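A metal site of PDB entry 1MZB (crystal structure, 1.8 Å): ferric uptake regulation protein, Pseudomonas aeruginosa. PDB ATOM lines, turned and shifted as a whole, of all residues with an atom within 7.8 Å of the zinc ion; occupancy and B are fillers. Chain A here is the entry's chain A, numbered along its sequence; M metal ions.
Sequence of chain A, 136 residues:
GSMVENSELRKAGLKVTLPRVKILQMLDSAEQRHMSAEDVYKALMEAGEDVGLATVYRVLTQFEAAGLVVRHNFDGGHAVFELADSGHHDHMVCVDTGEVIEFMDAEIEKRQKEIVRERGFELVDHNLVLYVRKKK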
ATOM      1  N   ARG A  33      11.897  26.651   3.949  1.00  0.00           N
ATOM      2  CA  ARG A  33      11.640  26.539   5.374  1.00  0.00           C
ATOM      3  C   ARG A  33      12.159  27.774   6.123  1.00  0.00           C
ATOM      4  O   ARG A  33      11.562  28.208   7.136  1.00  0.00           O
ATOM      5  CB  ARG A  33      12.307  25.273   5.928  1.00  0.00           C
ATOM      6  CG  ARG A  33      12.174  24.038   5.032  1.00  0.00           C
ATOM      7  CD  ARG A  33      12.486  22.768   5.828  1.00  0.00           C
ATOM      8  NE  ARG A  33      12.571  21.579   4.983  1.00  0.00           N
ATOM      9  CZ  ARG A  33      12.646  20.342   5.465  1.00  0.00           C
ATOM     10  NH1 ARG A  33      12.650  20.139   6.782  1.00  0.00           N
ATOM     11  NH2 ARG A  33      12.730  19.297   4.631  1.00  0.00           N
ATOM     12  N   HIS A  34      13.249  28.341   5.600  1.00  0.00           N
ATOM     13  CA  HIS A  34      13.910  29.512   6.190  1.00  0.00           C
ATOM     14  C   HIS A  34      13.924  30.713   5.244  1.00  0.00           C
ATOM     15  O   HIS A  34      14.894  30.984   4.536  1.00  0.00           O
ATOM     16  CB  HIS A  34      15.331  29.153   6.592  1.00  0.00           C
ATOM     17  CG  HIS A  34      15.409  27.910   7.414  1.00  0.00           C
ATOM     18  ND1 HIS A  34      15.648  26.679   6.845  1.00  0.00           N
ATOM     19  CD2 HIS A  34      15.184  27.750   8.741  1.00  0.00           C
ATOM     20  CE1 HIS A  34      15.550  25.797   7.823  1.00  0.00           C
ATOM     21  NE2 HIS A  34      15.274  26.394   9.001  1.00  0.00           N
ATOM     22  N   HIS A  72      16.859  34.189  12.764  1.00  0.00           N
ATOM     23  CA  HIS A  72      18.164  33.564  12.787  1.00  0.00           C
ATOM     24  C   HIS A  72      19.025  34.250  11.701  1.00  0.00           C
ATOM     25  O   HIS A  72      18.484  34.814  10.767  1.00  0.00           O
ATOM     26  CB  HIS A  72      18.075  32.088  12.364  1.00  0.00           C
ATOM     27  CG  HIS A  72      17.521  31.174  13.418  1.00  0.00           C
ATOM     28  ND1 HIS A  72      16.317  30.512  13.255  1.00  0.00           N
ATOM     29  CD2 HIS A  72      18.064  30.702  14.558  1.00  0.00           C
ATOM     30  CE1 HIS A  72      16.146  29.668  14.259  1.00  0.00           C
ATOM     31  NE2 HIS A  72      17.198  29.754  15.061  1.00  0.00           N
ATOM     32  N   PHE A  74      22.059  32.844   9.665  1.00  0.00           N
ATOM     33  CA  PHE A  74      22.969  31.710   9.473  1.00  0.00           C
ATOM     34  C   PHE A  74      24.202  31.962   8.618  1.00  0.00           C
ATOM     35  O   PHE A  74      25.248  31.331   8.860  1.00  0.00           O
ATOM     36  CB  PHE A  74      22.213  30.529   8.849  1.00  0.00           C
ATOM     37  CG  PHE A  74      21.058  30.020   9.695  1.00  0.00           C
ATOM     38  CD1 PHE A  74      21.277  29.556  10.993  1.00  0.00           C
ATOM     39  CD2 PHE A  74      19.776  29.931   9.142  1.00  0.00           C
ATOM     40  CE1 PHE A  74      20.211  28.970  11.737  1.00  0.00           C
ATOM     41  CE2 PHE A  74      18.718  29.375   9.880  1.00  0.00           C
ATOM     42  CZ  PHE A  74      18.933  28.896  11.169  1.00  0.00           C
ATOM     43  N   VAL A  80      16.825  35.236   8.623  1.00  0.00           N
ATOM     44  CA  VAL A  80      15.869  34.241   8.203  1.00  0.00           C
ATOM     45  C   VAL A  80      14.767  34.268   9.254  1.00  0.00           C
ATOM     46  O   VAL A  80      15.088  34.387  10.428  1.00  0.00           O
ATOM     47  CB  VAL A  80      16.520  32.852   8.229  1.00  0.00           C
ATOM     48  CG1 VAL A  80      15.492  31.758   8.418  1.00  0.00           C
ATOM     49  CG2 VAL A  80      17.292  32.667   6.919  1.00  0.00           C
ATOM     50  N   PHE A  81      13.498  34.132   8.852  1.00  0.00           N
ATOM     51  CA  PHE A  81      12.423  34.146   9.838  1.00  0.00           C
ATOM     52  C   PHE A  81      11.674  32.836   9.675  1.00  0.00           C
ATOM     53  O   PHE A  81      11.373  32.451   8.559  1.00  0.00           O
ATOM     54  CB  PHE A  81      11.449  35.296   9.561  1.00  0.00           C
ATOM     55  CG  PHE A  81      12.055  36.665   9.761  1.00  0.00           C
ATOM     56  CD1 PHE A  81      12.755  37.300   8.737  1.00  0.00           C
ATOM     57  CD2 PHE A  81      11.910  37.332  10.986  1.00  0.00           C
ATOM     58  CE1 PHE A  81      13.299  38.618   8.927  1.00  0.00           C
ATOM     59  CE2 PHE A  81      12.447  38.620  11.182  1.00  0.00           C
ATOM     60  CZ  PHE A  81      13.137  39.271  10.146  1.00  0.00           C
ATOM     61  N   GLU A  82      11.418  32.128  10.764  1.00  0.00           N
ATOM     62  CA  GLU A  82      10.695  30.856  10.641  1.00  0.00           C
ATOM     63  C   GLU A  82       9.731  30.764  11.800  1.00  0.00           C
ATOM     64  O   GLU A  82       9.934  31.394  12.817  1.00  0.00           O
ATOM     65  CB  GLU A  82      11.648  29.668  10.632  1.00  0.00           C
ATOM     66  CG  GLU A  82      12.598  29.574  11.841  1.00  0.00           C
ATOM     67  CD  GLU A  82      13.682  28.491  11.669  1.00  0.00           C
ATOM     68  OE1 GLU A  82      13.355  27.293  11.665  1.00  0.00           O
ATOM     69  OE2 GLU A  82      14.863  28.853  11.538  1.00  0.00           O
ATOM     70  N   LEU A  83       8.652  30.027  11.619  1.00  0.00           N
ATOM     71  CA  LEU A  83       7.706  29.896  12.703  1.00  0.00           C
ATOM     72  C   LEU A  83       8.355  29.284  13.936  1.00  0.00           C
ATOM     73  O   LEU A  83       9.347  28.521  13.853  1.00  0.00           O
ATOM     74  CB  LEU A  83       6.539  29.030  12.237  1.00  0.00           C
ATOM     75  CG  LEU A  83       5.748  29.651  11.108  1.00  0.00           C
ATOM     76  CD1 LEU A  83       4.744  28.603  10.588  1.00  0.00           C
ATOM     77  CD2 LEU A  83       5.013  30.931  11.612  1.00  0.00           C
ATOM     78  N   SER A  86       6.173  25.475  15.085  1.00  0.00           N
ATOM     79  CA  SER A  86       6.569  24.198  14.510  1.00  0.00           C
ATOM     80  C   SER A  86       7.376  23.380  15.519  1.00  0.00           C
ATOM     81  O   SER A  86       7.904  23.922  16.504  1.00  0.00           O
ATOM     82  CB  SER A  86       7.409  24.425  13.248  1.00  0.00           C
ATOM     83  OG  SER A  86       8.614  25.125  13.561  1.00  0.00           O
ATOM     84  N   GLY A  87       7.491  22.066  15.283  1.00  0.00           N
ATOM     85  CA  GLY A  87       8.269  21.234  16.180  1.00  0.00           C
ATOM     86  C   GLY A  87       9.631  21.893  16.335  1.00  0.00           C
ATOM     87  O   GLY A  87      10.081  22.616  15.442  1.00  0.00           O
ATOM     88  N   HIS A  88      10.288  21.661  17.464  1.00  0.00           N
ATOM     89  CA  HIS A  88      11.601  22.262  17.696  1.00  0.00           C
ATOM     90  C   HIS A  88      12.648  21.690  16.749  1.00  0.00           C
ATOM     91  O   HIS A  88      12.598  20.509  16.360  1.00  0.00           O
ATOM     92  CB  HIS A  88      12.065  22.021  19.137  1.00  0.00           C
ATOM     93  CG  HIS A  88      13.520  22.336  19.387  1.00  0.00           C
ATOM     94  ND1 HIS A  88      14.004  23.622  19.424  1.00  0.00           N
ATOM     95  CD2 HIS A  88      14.562  21.525  19.664  1.00  0.00           C
ATOM     96  CE1 HIS A  88      15.288  23.594  19.734  1.00  0.00           C
ATOM     97  NE2 HIS A  88      15.660  22.322  19.886  1.00  0.00           N
ATOM     98  N   HIS A  89      13.595  22.545  16.381  1.00  0.00           N
ATOM     99  CA  HIS A  89      14.675  22.169  15.486  1.00  0.00           C
ATOM    100  C   HIS A  89      15.871  23.080  15.707  1.00  0.00           C
ATOM    101  O   HIS A  89      15.732  24.283  15.915  1.00  0.00           O
ATOM    102  CB  HIS A  89      14.195  22.250  14.028  1.00  0.00           C
ATOM    103  N   ASP A  90      17.058  22.485  15.716  1.00  0.00           N
ATOM    104  CA  ASP A  90      18.271  23.264  15.845  1.00  0.00           C
ATOM    105  C   ASP A  90      18.792  23.190  14.421  1.00  0.00           C
ATOM    106  O   ASP A  90      18.117  22.649  13.575  1.00  0.00           O
ATOM    107  CB  ASP A  90      19.190  22.612  16.820  1.00  0.00           C
ATOM    108  CG  ASP A  90      18.540  22.536  18.214  1.00  0.00           C
ATOM    109  OD1 ASP A  90      18.072  23.570  18.703  1.00  0.00           O
ATOM    110  OD2 ASP A  90      18.527  21.480  18.762  1.00  0.00           O
ATOM    111  N   HIS A  91      19.976  23.707  14.138  1.00  0.00           N
ATOM    112  CA  HIS A  91      20.389  23.730  12.732  1.00  0.00           C
ATOM    113  C   HIS A  91      21.836  23.420  12.463  1.00  0.00           C
ATOM    114  O   HIS A  91      22.705  23.801  13.253  1.00  0.00           O
ATOM    115  CB  HIS A  91      20.130  25.145  12.130  1.00  0.00           C
ATOM    116  CG  HIS A  91      18.709  25.623  12.221  1.00  0.00           C
ATOM    117  ND1 HIS A  91      18.181  26.134  13.389  1.00  0.00           N
ATOM    118  CD2 HIS A  91      17.754  25.605  11.272  1.00  0.00           C
ATOM    119  CE1 HIS A  91      16.927  26.404  13.114  1.00  0.00           C
ATOM    120  NE2 HIS A  91      16.627  26.099  11.871  1.00  0.00           N
ATOM    121  N   VAL A 100      21.162  25.109   4.898  1.00  0.00           N
ATOM    122  CA  VAL A 100      20.737  24.932   6.299  1.00  0.00           C
ATOM    123  C   VAL A 100      19.998  23.625   6.414  1.00  0.00           C
ATOM    124  O   VAL A 100      19.042  23.352   5.641  1.00  0.00           O
ATOM    125  CB  VAL A 100      19.812  26.073   6.728  1.00  0.00           C
ATOM    126  CG1 VAL A 100      19.320  25.862   8.160  1.00  0.00           C
ATOM    127  CG2 VAL A 100      20.588  27.415   6.612  1.00  0.00           C
ATOM    128  N   ILE A 101      20.413  22.834   7.396  1.00  0.00           N
ATOM    129  CA  ILE A 101      19.847  21.508   7.655  1.00  0.00           C
ATOM    130  C   ILE A 101      19.303  21.487   9.086  1.00  0.00           C
ATOM    131  O   ILE A 101      20.040  21.659  10.051  1.00  0.00           O
ATOM    132  CB  ILE A 101      20.961  20.429   7.513  1.00  0.00           C
ATOM    133  CG1 ILE A 101      21.523  20.456   6.092  1.00  0.00           C
ATOM    134  CG2 ILE A 101      20.417  19.036   7.897  1.00  0.00           C
ATOM    135  CD1 ILE A 101      22.843  19.734   5.946  1.00  0.00           C
ATOM    136  N   GLU A 102      17.990  21.290   9.223  1.00  0.00           N
ATOM    137  CA  GLU A 102      17.407  21.199  10.566  1.00  0.00           C
ATOM    138  C   GLU A 102      17.646  19.806  11.172  1.00  0.00           C
ATOM    139  O   GLU A 102      17.717  18.786  10.458  1.00  0.00           O
ATOM    140  CB  GLU A 102      15.893  21.443  10.542  1.00  0.00           C
ATOM    141  CG  GLU A 102      15.485  22.885  10.281  1.00  0.00           C
ATOM    142  CD  GLU A 102      14.001  23.128  10.525  1.00  0.00           C
ATOM    143  OE1 GLU A 102      13.214  22.156  10.405  1.00  0.00           O
ATOM    144  OE2 GLU A 102      13.614  24.288  10.800  1.00  0.00           O
ATOM    145  N   PHE A 103      17.781  19.755  12.495  1.00  0.00           N
ATOM    146  CA  PHE A 103      17.923  18.480  13.196  1.00  0.00           C
ATOM    147  C   PHE A 103      17.375  18.669  14.588  1.00  0.00           C
ATOM    148  O   PHE A 103      17.178  19.795  15.048  1.00  0.00           O
ATOM    149  CB  PHE A 103      19.376  18.002  13.238  1.00  0.00           C
ATOM    150  CG  PHE A 103      20.258  18.779  14.184  1.00  0.00           C
ATOM    151  CD1 PHE A 103      20.886  19.955  13.781  1.00  0.00           C
ATOM    152  CD2 PHE A 103      20.458  18.320  15.469  1.00  0.00           C
ATOM    153  CE1 PHE A 103      21.719  20.669  14.656  1.00  0.00           C
ATOM    154  CE2 PHE A 103      21.283  19.011  16.371  1.00  0.00           C
ATOM    155  CZ  PHE A 103      21.916  20.194  15.957  1.00  0.00           C
HETATM  156 ZN    ZN M   1      14.813  26.077  10.925  1.00  0.00          ZN
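OE2 of Glu 82 is in hydrogen-bond range of ND1 of His 72 (2.8 Å).
The nearest printed residue that does not touch the zinc ion is His 89 (5.0 Å).
The zinc ion is bound by NE2 of His 34 (2.0 Å), OE1 of Glu 82 (2.0 Å), NE2 of His 91 (2.0 Å) and OE2 of Glu 102 (2.2 Å).
Slightly farther from the zinc ion lies OE2 of Glu 82 (2.8 Å).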
